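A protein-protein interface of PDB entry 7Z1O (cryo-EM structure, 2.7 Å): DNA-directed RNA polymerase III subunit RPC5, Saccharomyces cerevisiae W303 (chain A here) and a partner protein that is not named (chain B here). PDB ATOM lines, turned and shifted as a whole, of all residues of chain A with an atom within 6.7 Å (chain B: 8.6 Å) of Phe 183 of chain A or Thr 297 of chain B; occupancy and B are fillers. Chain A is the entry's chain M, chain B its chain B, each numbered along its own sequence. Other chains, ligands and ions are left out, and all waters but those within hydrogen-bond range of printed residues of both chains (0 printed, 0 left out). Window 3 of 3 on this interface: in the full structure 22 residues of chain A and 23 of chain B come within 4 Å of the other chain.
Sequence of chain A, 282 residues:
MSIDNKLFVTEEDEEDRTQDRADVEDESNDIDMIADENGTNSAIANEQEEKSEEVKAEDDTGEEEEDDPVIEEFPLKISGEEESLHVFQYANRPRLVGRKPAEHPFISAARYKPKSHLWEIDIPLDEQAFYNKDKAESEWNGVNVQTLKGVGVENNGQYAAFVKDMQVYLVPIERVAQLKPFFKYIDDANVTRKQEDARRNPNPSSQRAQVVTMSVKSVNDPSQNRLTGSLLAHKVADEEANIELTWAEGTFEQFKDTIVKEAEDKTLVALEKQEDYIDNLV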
ATOM      1  N   GLN A 146       9.170   7.808  24.395  1.00  0.00           N
ATOM      2  CA  GLN A 146       9.199   9.152  23.839  1.00  0.00           C
ATOM      3  C   GLN A 146      10.634   9.660  23.856  1.00  0.00           C
ATOM      4  O   GLN A 146      11.327   9.552  24.872  1.00  0.00           O
ATOM      5  CB  GLN A 146       8.288  10.097  24.624  1.00  0.00           C
ATOM      6  CG  GLN A 146       8.378   9.955  26.134  1.00  0.00           C
ATOM      7  CD  GLN A 146       7.832  11.165  26.861  1.00  0.00           C
ATOM      8  OE1 GLN A 146       7.678  12.237  26.276  1.00  0.00           O
ATOM      9  NE2 GLN A 146       7.536  11.001  28.145  1.00  0.00           N
ATOM     10  N   THR A 147      11.084  10.193  22.729  1.00  0.00           N
ATOM     11  CA  THR A 147      12.454  10.657  22.595  1.00  0.00           C
ATOM     12  C   THR A 147      12.498  12.180  22.569  1.00  0.00           C
ATOM     13  O   THR A 147      11.602  12.836  22.030  1.00  0.00           O
ATOM     14  CB  THR A 147      13.117  10.065  21.344  1.00  0.00           C
ATOM     15  OG1 THR A 147      14.462  10.544  21.238  1.00  0.00           O
ATOM     16  CG2 THR A 147      12.342  10.403  20.085  1.00  0.00           C
ATOM     17  N   PRO A 181      10.467  17.351  22.103  1.00  0.00           N
ATOM     18  CA  PRO A 181       9.973  16.049  21.634  1.00  0.00           C
ATOM     19  C   PRO A 181      10.313  15.785  20.174  1.00  0.00           C
ATOM     20  O   PRO A 181      10.269  16.681  19.330  1.00  0.00           O
ATOM     21  CB  PRO A 181       8.457  16.151  21.842  1.00  0.00           C
ATOM     22  CG  PRO A 181       8.293  17.159  22.911  1.00  0.00           C
ATOM     23  CD  PRO A 181       9.390  18.154  22.711  1.00  0.00           C
ATOM     24  N   PHE A 182      10.659  14.533  19.890  1.00  0.00           N
ATOM     25  CA  PHE A 182      11.016  14.081  18.557  1.00  0.00           C
ATOM     26  C   PHE A 182      10.117  12.907  18.203  1.00  0.00           C
ATOM     27  O   PHE A 182       9.770  12.097  19.068  1.00  0.00           O
ATOM     28  CB  PHE A 182      12.494  13.680  18.493  1.00  0.00           C
ATOM     29  CG  PHE A 182      13.015  13.476  17.102  1.00  0.00           C
ATOM     30  CD1 PHE A 182      12.605  14.295  16.066  1.00  0.00           C
ATOM     31  CD2 PHE A 182      13.935  12.475  16.836  1.00  0.00           C
ATOM     32  CE1 PHE A 182      13.091  14.110  14.785  1.00  0.00           C
ATOM     33  CE2 PHE A 182      14.424  12.288  15.561  1.00  0.00           C
ATOM     34  CZ  PHE A 182      14.002  13.105  14.534  1.00  0.00           C
ATOM     35  N   PHE A 183       9.727  12.828  16.938  1.00  0.00           N
ATOM     36  CA  PHE A 183       8.730  11.874  16.468  1.00  0.00           C
ATOM     37  C   PHE A 183       9.279  11.074  15.299  1.00  0.00           C
ATOM     38  O   PHE A 183       8.686  11.011  14.220  1.00  0.00           O
ATOM     39  CB  PHE A 183       7.433  12.585  16.104  1.00  0.00           C
ATOM     40  CG  PHE A 183       6.799  13.308  17.256  1.00  0.00           C
ATOM     41  CD1 PHE A 183       6.610  12.670  18.468  1.00  0.00           C
ATOM     42  CD2 PHE A 183       6.399  14.626  17.128  1.00  0.00           C
ATOM     43  CE1 PHE A 183       6.030  13.331  19.531  1.00  0.00           C
ATOM     44  CE2 PHE A 183       5.819  15.293  18.188  1.00  0.00           C
ATOM     45  CZ  PHE A 183       5.636  14.643  19.391  1.00  0.00           C
ATOM     46  N   LYS A 184      10.458  10.476  15.505  1.00  0.00           N
ATOM     47  CA  LYS A 184      11.155   9.767  14.436  1.00  0.00           C
ATOM     48  C   LYS A 184      10.348   8.603  13.873  1.00  0.00           C
ATOM     49  O   LYS A 184      10.576   8.192  12.730  1.00  0.00           O
ATOM     50  CB  LYS A 184      12.511   9.265  14.939  1.00  0.00           C
ATOM     51  CG  LYS A 184      12.424   8.206  16.024  1.00  0.00           C
ATOM     52  CD  LYS A 184      13.804   7.818  16.526  1.00  0.00           C
ATOM     53  CE  LYS A 184      14.570   7.032  15.475  1.00  0.00           C
ATOM     54  NZ  LYS A 184      13.934   5.717  15.192  1.00  0.00           N
ATOM     55  N   TYR A 185       9.403   8.058  14.645  1.00  0.00           N
ATOM     56  CA  TYR A 185       8.550   7.009  14.098  1.00  0.00           C
ATOM     57  C   TYR A 185       7.593   7.557  13.046  1.00  0.00           C
ATOM     58  O   TYR A 185       7.287   6.860  12.074  1.00  0.00           O
ATOM     59  CB  TYR A 185       7.781   6.295  15.211  1.00  0.00           C
ATOM     60  CG  TYR A 185       7.170   7.191  16.262  1.00  0.00           C
ATOM     61  CD1 TYR A 185       5.924   7.769  16.073  1.00  0.00           C
ATOM     62  CD2 TYR A 185       7.829   7.434  17.459  1.00  0.00           C
ATOM     63  CE1 TYR A 185       5.359   8.579  17.038  1.00  0.00           C
ATOM     64  CE2 TYR A 185       7.272   8.240  18.429  1.00  0.00           C
ATOM     65  CZ  TYR A 185       6.038   8.810  18.213  1.00  0.00           C
ATOM     66  OH  TYR A 185       5.483   9.615  19.179  1.00  0.00           O
ATOM     67  N   ILE A 186       7.134   8.801  13.207  1.00  0.00           N
ATOM     68  CA  ILE A 186       6.289   9.425  12.189  1.00  0.00           C
ATOM     69  C   ILE A 186       7.070   9.609  10.893  1.00  0.00           C
ATOM     70  O   ILE A 186       6.575   9.311   9.799  1.00  0.00           O
ATOM     71  CB  ILE A 186       5.723  10.760  12.706  1.00  0.00           C
ATOM     72  CG1 ILE A 186       4.755  10.516  13.864  1.00  0.00           C
ATOM     73  CG2 ILE A 186       5.023  11.519  11.593  1.00  0.00           C
ATOM     74  CD1 ILE A 186       4.199  11.782  14.472  1.00  0.00           C
ATOM     75  N   ASP A 187       8.313  10.089  11.002  1.00  0.00           N
ATOM     76  CA  ASP A 187       9.154  10.263   9.820  1.00  0.00           C
ATOM     77  C   ASP A 187       9.480   8.926   9.167  1.00  0.00           C
ATOM     78  O   ASP A 187       9.505   8.819   7.934  1.00  0.00           O
ATOM     79  CB  ASP A 187      10.438  11.002  10.198  1.00  0.00           C
ATOM     80  CG  ASP A 187      10.293  12.508  10.108  1.00  0.00           C
ATOM     81  OD1 ASP A 187       9.511  12.983   9.258  1.00  0.00           O
ATOM     82  OD2 ASP A 187      10.961  13.218  10.889  1.00  0.00           O
ATOM     83  N   ASP A 188       9.735   7.896   9.978  1.00  0.00           N
ATOM     84  CA  ASP A 188      10.013   6.569   9.435  1.00  0.00           C
ATOM     85  C   ASP A 188       8.800   6.001   8.709  1.00  0.00           C
ATOM     86  O   ASP A 188       8.933   5.421   7.626  1.00  0.00           O
ATOM     87  CB  ASP A 188      10.458   5.627  10.554  1.00  0.00           C
ATOM     88  CG  ASP A 188      10.893   4.272  10.034  1.00  0.00           C
ATOM     89  OD1 ASP A 188      11.995   4.182   9.452  1.00  0.00           O
ATOM     90  OD2 ASP A 188      10.134   3.296  10.208  1.00  0.00           O
ATOM     91  N   ASN A 190       6.407   7.780   7.325  1.00  0.00           N
ATOM     92  CA  ASN A 190       6.223   8.576   6.115  1.00  0.00           C
ATOM     93  C   ASN A 190       7.193   8.158   5.015  1.00  0.00           C
ATOM     94  O   ASN A 190       6.797   8.025   3.851  1.00  0.00           O
ATOM     95  CB  ASN A 190       6.385  10.061   6.435  1.00  0.00           C
ATOM     96  CG  ASN A 190       5.107  10.687   6.955  1.00  0.00           C
ATOM     97  OD1 ASN A 190       5.049  11.159   8.090  1.00  0.00           O
ATOM     98  ND2 ASN A 190       4.071  10.694   6.124  1.00  0.00           N
ATOM     99  N   ALA B 254       2.001  28.291  12.156  1.00  0.00           N
ATOM    100  CA  ALA B 254       2.345  27.116  12.949  1.00  0.00           C
ATOM    101  C   ALA B 254       3.352  26.239  12.216  1.00  0.00           C
ATOM    102  O   ALA B 254       4.284  25.709  12.828  1.00  0.00           O
ATOM    103  CB  ALA B 254       1.086  26.321  13.291  1.00  0.00           C
ATOM    104  N   ILE B 255       3.195  26.100  10.899  1.00  0.00           N
ATOM    105  CA  ILE B 255       4.110  25.277  10.114  1.00  0.00           C
ATOM    106  C   ILE B 255       5.501  25.899  10.077  1.00  0.00           C
ATOM    107  O   ILE B 255       6.512  25.208  10.259  1.00  0.00           O
ATOM    108  CB  ILE B 255       3.548  25.062   8.699  1.00  0.00           C
ATOM    109  CG1 ILE B 255       2.284  24.209   8.763  1.00  0.00           C
ATOM    110  CG2 ILE B 255       4.581  24.412   7.797  1.00  0.00           C
ATOM    111  CD1 ILE B 255       1.450  24.287   7.523  1.00  0.00           C
ATOM    112  N   LEU B 257       6.758  27.962  12.198  1.00  0.00           N
ATOM    113  CA  LEU B 257       7.352  27.879  13.527  1.00  0.00           C
ATOM    114  C   LEU B 257       7.797  26.458  13.849  1.00  0.00           C
ATOM    115  O   LEU B 257       8.762  26.268  14.597  1.00  0.00           O
ATOM    116  CB  LEU B 257       6.367  28.388  14.578  1.00  0.00           C
ATOM    117  CG  LEU B 257       6.458  29.885  14.877  1.00  0.00           C
ATOM    118  CD1 LEU B 257       5.344  30.322  15.809  1.00  0.00           C
ATOM    119  CD2 LEU B 257       7.814  30.234  15.458  1.00  0.00           C
ATOM    120  N   LYS B 258       7.111  25.453  13.298  1.00  0.00           N
ATOM    121  CA  LYS B 258       7.520  24.069  13.509  1.00  0.00           C
ATOM    122  C   LYS B 258       8.770  23.720  12.715  1.00  0.00           C
ATOM    123  O   LYS B 258       9.560  22.876  13.149  1.00  0.00           O
ATOM    124  CB  LYS B 258       6.380  23.121  13.146  1.00  0.00           C
ATOM    125  CG  LYS B 258       5.514  22.727  14.326  1.00  0.00           C
ATOM    126  CD  LYS B 258       4.365  21.839  13.898  1.00  0.00           C
ATOM    127  CE  LYS B 258       3.257  21.856  14.931  1.00  0.00           C
ATOM    128  NZ  LYS B 258       3.752  21.448  16.272  1.00  0.00           N
ATOM    129  N   ALA B 259       8.962  24.346  11.553  1.00  0.00           N
ATOM    130  CA  ALA B 259      10.182  24.133  10.783  1.00  0.00           C
ATOM    131  C   ALA B 259      11.413  24.659  11.505  1.00  0.00           C
ATOM    132  O   ALA B 259      12.527  24.215  11.212  1.00  0.00           O
ATOM    133  CB  ALA B 259      10.067  24.794   9.411  1.00  0.00           C
ATOM    134  N   CYS B 260      11.233  25.589  12.432  1.00  0.00           N
ATOM    135  CA  CYS B 260      12.307  26.087  13.275  1.00  0.00           C
ATOM    136  C   CYS B 260      12.437  25.173  14.496  1.00  0.00           C
ATOM    137  O   CYS B 260      11.920  24.053  14.504  1.00  0.00           O
ATOM    138  CB  CYS B 260      12.043  27.549  13.632  1.00  0.00           C
ATOM    139  SG  CYS B 260      11.934  28.653  12.207  1.00  0.00           S
ATOM    140  N   ILE B 262      11.151  25.046  17.363  1.00  0.00           N
ATOM    141  CA  ILE B 262       9.960  24.693  18.128  1.00  0.00           C
ATOM    142  C   ILE B 262       9.264  23.505  17.483  1.00  0.00           C
ATOM    143  O   ILE B 262       9.083  23.460  16.261  1.00  0.00           O
ATOM    144  CB  ILE B 262       9.020  25.902  18.231  1.00  0.00           C
ATOM    145  CG1 ILE B 262       9.796  27.138  18.675  1.00  0.00           C
ATOM    146  CG2 ILE B 262       7.889  25.615  19.193  1.00  0.00           C
ATOM    147  CD1 ILE B 262       9.055  28.417  18.433  1.00  0.00           C
ATOM    148  N   LEU B 263       8.879  22.523  18.303  1.00  0.00           N
ATOM    149  CA  LEU B 263       8.165  21.343  17.826  1.00  0.00           C
ATOM    150  C   LEU B 263       6.865  21.068  18.574  1.00  0.00           C
ATOM    151  O   LEU B 263       6.228  20.041  18.318  1.00  0.00           O
ATOM    152  CB  LEU B 263       9.050  20.093  17.895  1.00  0.00           C
ATOM    153  CG  LEU B 263      10.052  19.748  16.787  1.00  0.00           C
ATOM    154  CD1 LEU B 263       9.300  19.478  15.494  1.00  0.00           C
ATOM    155  CD2 LEU B 263      11.145  20.782  16.576  1.00  0.00           C
ATOM    156  N   SER B 264       6.447  21.943  19.485  1.00  0.00           N
ATOM    157  CA  SER B 264       5.241  21.717  20.271  1.00  0.00           C
ATOM    158  C   SER B 264       4.310  22.916  20.166  1.00  0.00           C
ATOM    159  O   SER B 264       4.763  24.061  20.070  1.00  0.00           O
ATOM    160  CB  SER B 264       5.581  21.440  21.737  1.00  0.00           C
ATOM    161  OG  SER B 264       5.736  22.641  22.464  1.00  0.00           O
ATOM    162  N   ASP B 265       3.001  22.643  20.179  1.00  0.00           N
ATOM    163  CA  ASP B 265       2.017  23.708  20.008  1.00  0.00           C
ATOM    164  C   ASP B 265       1.893  24.569  21.259  1.00  0.00           C
ATOM    165  O   ASP B 265       1.613  25.771  21.167  1.00  0.00           O
ATOM    166  CB  ASP B 265       0.660  23.118  19.631  1.00  0.00           C
ATOM    167  CG  ASP B 265       0.593  22.698  18.178  1.00  0.00           C
ATOM    168  OD1 ASP B 265      -0.319  21.922  17.821  1.00  0.00           O
ATOM    169  OD2 ASP B 265       1.454  23.144  17.391  1.00  0.00           O
ATOM    170  N   SER B 290      -1.852  22.927  11.841  1.00  0.00           N
ATOM    171  CA  SER B 290      -0.852  21.870  11.897  1.00  0.00           C
ATOM    172  C   SER B 290      -1.506  20.499  11.986  1.00  0.00           C
ATOM    173  O   SER B 290      -0.957  19.514  11.479  1.00  0.00           O
ATOM    174  CB  SER B 290       0.094  22.097  13.078  1.00  0.00           C
ATOM    175  OG  SER B 290      -0.603  22.092  14.313  1.00  0.00           O
ATOM    176  N   ASP B 294      -1.598  17.650   8.738  1.00  0.00           N
ATOM    177  CA  ASP B 294      -0.823  16.498   9.210  1.00  0.00           C
ATOM    178  C   ASP B 294       0.681  16.765   9.149  1.00  0.00           C
ATOM    179  O   ASP B 294       1.466  15.941   8.677  1.00  0.00           O
ATOM    180  CB  ASP B 294      -1.191  15.232   8.432  1.00  0.00           C
ATOM    181  CG  ASP B 294      -0.950  13.966   9.231  1.00  0.00           C
ATOM    182  OD1 ASP B 294      -0.273  14.039  10.279  1.00  0.00           O
ATOM    183  OD2 ASP B 294      -1.440  12.897   8.811  1.00  0.00           O
ATOM    184  N   ILE B 295       1.080  17.938   9.631  1.00  0.00           N
ATOM    185  CA  ILE B 295       2.483  18.311   9.752  1.00  0.00           C
ATOM    186  C   ILE B 295       2.804  18.344  11.238  1.00  0.00           C
ATOM    187  O   ILE B 295       2.239  19.150  11.987  1.00  0.00           O
ATOM    188  CB  ILE B 295       2.778  19.659   9.085  1.00  0.00           C
ATOM    189  CG1 ILE B 295       2.715  19.515   7.566  1.00  0.00           C
ATOM    190  CG2 ILE B 295       4.140  20.178   9.508  1.00  0.00           C
ATOM    191  CD1 ILE B 295       2.513  20.814   6.847  1.00  0.00           C
ATOM    192  N   TYR B 296       3.706  17.464  11.673  1.00  0.00           N
ATOM    193  CA  TYR B 296       3.974  17.305  13.092  1.00  0.00           C
ATOM    194  C   TYR B 296       5.453  17.232  13.441  1.00  0.00           C
ATOM    195  O   TYR B 296       5.781  17.208  14.631  1.00  0.00           O
ATOM    196  CB  TYR B 296       3.281  16.042  13.623  1.00  0.00           C
ATOM    197  CG  TYR B 296       1.823  16.256  13.947  1.00  0.00           C
ATOM    198  CD1 TYR B 296       0.829  15.789  13.098  1.00  0.00           C
ATOM    199  CD2 TYR B 296       1.441  16.970  15.068  1.00  0.00           C
ATOM    200  CE1 TYR B 296      -0.508  15.992  13.384  1.00  0.00           C
ATOM    201  CE2 TYR B 296       0.109  17.179  15.365  1.00  0.00           C
ATOM    202  CZ  TYR B 296      -0.860  16.691  14.519  1.00  0.00           C
ATOM    203  OH  TYR B 296      -2.188  16.902  14.811  1.00  0.00           O
ATOM    204  N   THR B 297       6.348  17.195  12.458  1.00  0.00           N
ATOM    205  CA  THR B 297       7.780  17.139  12.699  1.00  0.00           C
ATOM    206  C   THR B 297       8.461  18.283  11.966  1.00  0.00           C
ATOM    207  O   THR B 297       7.870  18.935  11.101  1.00  0.00           O
ATOM    208  CB  THR B 297       8.387  15.805  12.247  1.00  0.00           C
ATOM    209  OG1 THR B 297       7.951  15.504  10.917  1.00  0.00           O
ATOM    210  CG2 THR B 297       7.961  14.689  13.175  1.00  0.00           C
ATOM    211  N   GLN B 298       9.719  18.527  12.337  1.00  0.00           N
ATOM    212  CA  GLN B 298      10.498  19.567  11.675  1.00  0.00           C
ATOM    213  C   GLN B 298      10.755  19.214  10.217  1.00  0.00           C
ATOM    214  O   GLN B 298      10.689  20.082   9.337  1.00  0.00           O
ATOM    215  CB  GLN B 298      11.815  19.787  12.420  1.00  0.00           C
ATOM    216  CG  GLN B 298      12.670  20.908  11.856  1.00  0.00           C
ATOM    217  CD  GLN B 298      13.830  21.269  12.759  1.00  0.00           C
ATOM    218  OE1 GLN B 298      14.204  20.503  13.645  1.00  0.00           O
ATOM    219  NE2 GLN B 298      14.408  22.443  12.538  1.00  0.00           N
ATOM    220  N   GLN B 299      11.048  17.939   9.940  1.00  0.00           N
ATOM    221  CA  GLN B 299      11.306  17.515   8.567  1.00  0.00           C
ATOM    222  C   GLN B 299      10.063  17.655   7.698  1.00  0.00           C
ATOM    223  O   GLN B 299      10.158  18.064   6.537  1.00  0.00           O
ATOM    224  CB  GLN B 299      11.815  16.076   8.544  1.00  0.00           C
ATOM    225  CG  GLN B 299      13.194  15.896   9.148  1.00  0.00           C
ATOM    226  CD  GLN B 299      13.681  14.464   9.060  1.00  0.00           C
ATOM    227  OE1 GLN B 299      12.969  13.583   8.578  1.00  0.00           O
ATOM    228  NE2 GLN B 299      14.900  14.224   9.529  1.00  0.00           N
ATOM    229  N   GLN B 300       8.889  17.319   8.239  1.00  0.00           N
ATOM    230  CA  GLN B 300       7.650  17.464   7.478  1.00  0.00           C
ATOM    231  C   GLN B 300       7.359  18.926   7.165  1.00  0.00           C
ATOM    232  O   GLN B 300       6.932  19.260   6.052  1.00  0.00           O
ATOM    233  CB  GLN B 300       6.486  16.845   8.252  1.00  0.00           C
ATOM    234  CG  GLN B 300       6.303  15.357   8.024  1.00  0.00           C
ATOM    235  CD  GLN B 300       5.136  14.791   8.806  1.00  0.00           C
ATOM    236  OE1 GLN B 300       4.900  15.170   9.951  1.00  0.00           O
ATOM    237  NE2 GLN B 300       4.398  13.878   8.187  1.00  0.00           N
ATOM    238  N   ALA B 301       7.586  19.813   8.136  1.00  0.00           N
ATOM    239  CA  ALA B 301       7.382  21.238   7.904  1.00  0.00           C
ATOM    240  C   ALA B 301       8.360  21.773   6.868  1.00  0.00           C
ATOM    241  O   ALA B 301       7.996  22.610   6.033  1.00  0.00           O
ATOM    242  CB  ALA B 301       7.514  22.006   9.219  1.00  0.00           C
ATOM    243  N   LEU B 302       9.610  21.304   6.908  1.00  0.00           N
ATOM    244  CA  LEU B 302      10.583  21.721   5.904  1.00  0.00           C
ATOM    245  C   LEU B 302      10.214  21.201   4.519  1.00  0.00           C
ATOM    246  O   LEU B 302      10.400  21.905   3.520  1.00  0.00           O
ATOM    247  CB  LEU B 302      11.983  21.267   6.310  1.00  0.00           C
ATOM    248  CG  LEU B 302      12.570  22.074   7.472  1.00  0.00           C
ATOM    249  CD1 LEU B 302      13.674  21.305   8.175  1.00  0.00           C
ATOM    250  CD2 LEU B 302      13.072  23.419   6.991  1.00  0.00           C
ATOM    251  N   GLU B 303       9.679  19.976   4.438  1.00  0.00           N
ATOM    252  CA  GLU B 303       9.129  19.475   3.178  1.00  0.00           C
ATOM    253  C   GLU B 303       8.023  20.382   2.658  1.00  0.00           C
ATOM    254  O   GLU B 303       8.005  20.746   1.477  1.00  0.00           O
ATOM    255  CB  GLU B 303       8.573  18.059   3.351  1.00  0.00           C
ATOM    256  CG  GLU B 303       9.555  16.949   3.651  1.00  0.00           C
ATOM    257  CD  GLU B 303      10.486  16.678   2.497  1.00  0.00           C
ATOM    258  OE1 GLU B 303      10.060  16.863   1.338  1.00  0.00           O
ATOM    259  OE2 GLU B 303      11.625  16.236   2.747  1.00  0.00           O
ATOM    260  N   TYR B 304       7.084  20.743   3.534  1.00  0.00           N
ATOM    261  CA  TYR B 304       5.944  21.548   3.111  1.00  0.00           C
ATOM    262  C   TYR B 304       6.385  22.928   2.645  1.00  0.00           C
ATOM    263  O   TYR B 304       5.844  23.466   1.671  1.00  0.00           O
ATOM    264  CB  TYR B 304       4.937  21.664   4.253  1.00  0.00           C
ATOM    265  CG  TYR B 304       3.694  22.446   3.907  1.00  0.00           C
ATOM    266  CD1 TYR B 304       2.629  21.836   3.260  1.00  0.00           C
ATOM    267  CD2 TYR B 304       3.576  23.790   4.238  1.00  0.00           C
ATOM    268  CE1 TYR B 304       1.486  22.540   2.947  1.00  0.00           C
ATOM    269  CE2 TYR B 304       2.436  24.504   3.925  1.00  0.00           C
ATOM    270  CZ  TYR B 304       1.395  23.871   3.281  1.00  0.00           C
ATOM    271  OH  TYR B 304       0.255  24.570   2.966  1.00  0.00           O
ATOM    272  N   LEU B 320      13.920  18.707   0.986  1.00  0.00           N
ATOM    273  CA  LEU B 320      14.153  18.990   2.400  1.00  0.00           C
ATOM    274  C   LEU B 320      15.305  19.973   2.577  1.00  0.00           C
ATOM    275  O   LEU B 320      15.220  20.905   3.387  1.00  0.00           O
ATOM    276  CB  LEU B 320      14.413  17.677   3.145  1.00  0.00           C
ATOM    277  CG  LEU B 320      14.534  17.581   4.668  1.00  0.00           C
ATOM    278  CD1 LEU B 320      14.082  16.203   5.117  1.00  0.00           C
ATOM    279  CD2 LEU B 320      15.959  17.783   5.107  1.00  0.00           C
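Hydrophobic or aromatic side chains of chain B that line the printed part of chain A: Leu 263. Hydrophobic or aromatic side chains of chain A within 4 Å of the printed part of chain B: Phe 183. Among the printed residues, 6 pairs touch across the chains.
N of Tyr 296 of chain B is in hydrogen-bond range of OE1 of Gln 300 of chain B, 3.1 Å away. O of Ile 186 of chain A lies close to OD1 of Asn 190 of chain A (2.9 Å). The side-chain amide oxygen of Gln 300 of chain B sits at hydrogen-bond distance from the side-chain hydroxyl of Thr 297 of chain B (3.2 Å).
The side-chain amide oxygen of Asn 190 of chain A is in hydrogen-bond range of the side-chain amide nitrogen of Gln 300 of chain B (2.8 Å). The side-chain carboxylate (OD2) of Asp 187 of chain A sits close to the side-chain amide oxygen (OE1) of Gln 299 of chain B (3.1 Å). The side-chain carboxylate (OD1) of Asp 187 of chain A sits at hydrogen-bond distance from the side-chain hydroxyl (OG1) of Thr 297 of chain B (3.4 Å).
Among the printed residues, pairs that only touch across the chains: Phe 183 of chain A with Tyr 296 of chain B, Phe 183 of chain A with Thr 297 of chain B and Pro 181 of chain A with Leu 263 of chain B.
Of the printed residues of chain B, Phe 183 of chain A touches Tyr 296 (3.6 Å) and Thr 297 (3.6 Å). Of the printed residues of chain A, Thr 297 of chain B touches Phe 183 (3.6 Å) and Asp 187 (3.4 Å). Of the printed residues of chain A, Tyr 296 of chain B touches Phe 183. Printed residues of chain B within 4 Å of Pro 181 of chain A: Leu 263 (3.9 Å). Printed residues of chain A within 4 Å of Gln 300 of chain B: Asn 190. Of the printed residues of chain B, Asp 187 of chain A touches Thr 297 (3.4 Å) and Gln 299 (3.1 Å). Glu 303 of chain B touches none of the printed residues of chain A. The nearest residue of chain B that does not touch Phe 183 of chain A is Leu 263 of chain B (4.8 Å). The nearest residue of chain A that does not touch Thr 297 of chain B is Ile 186 of chain A (4.5 Å).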
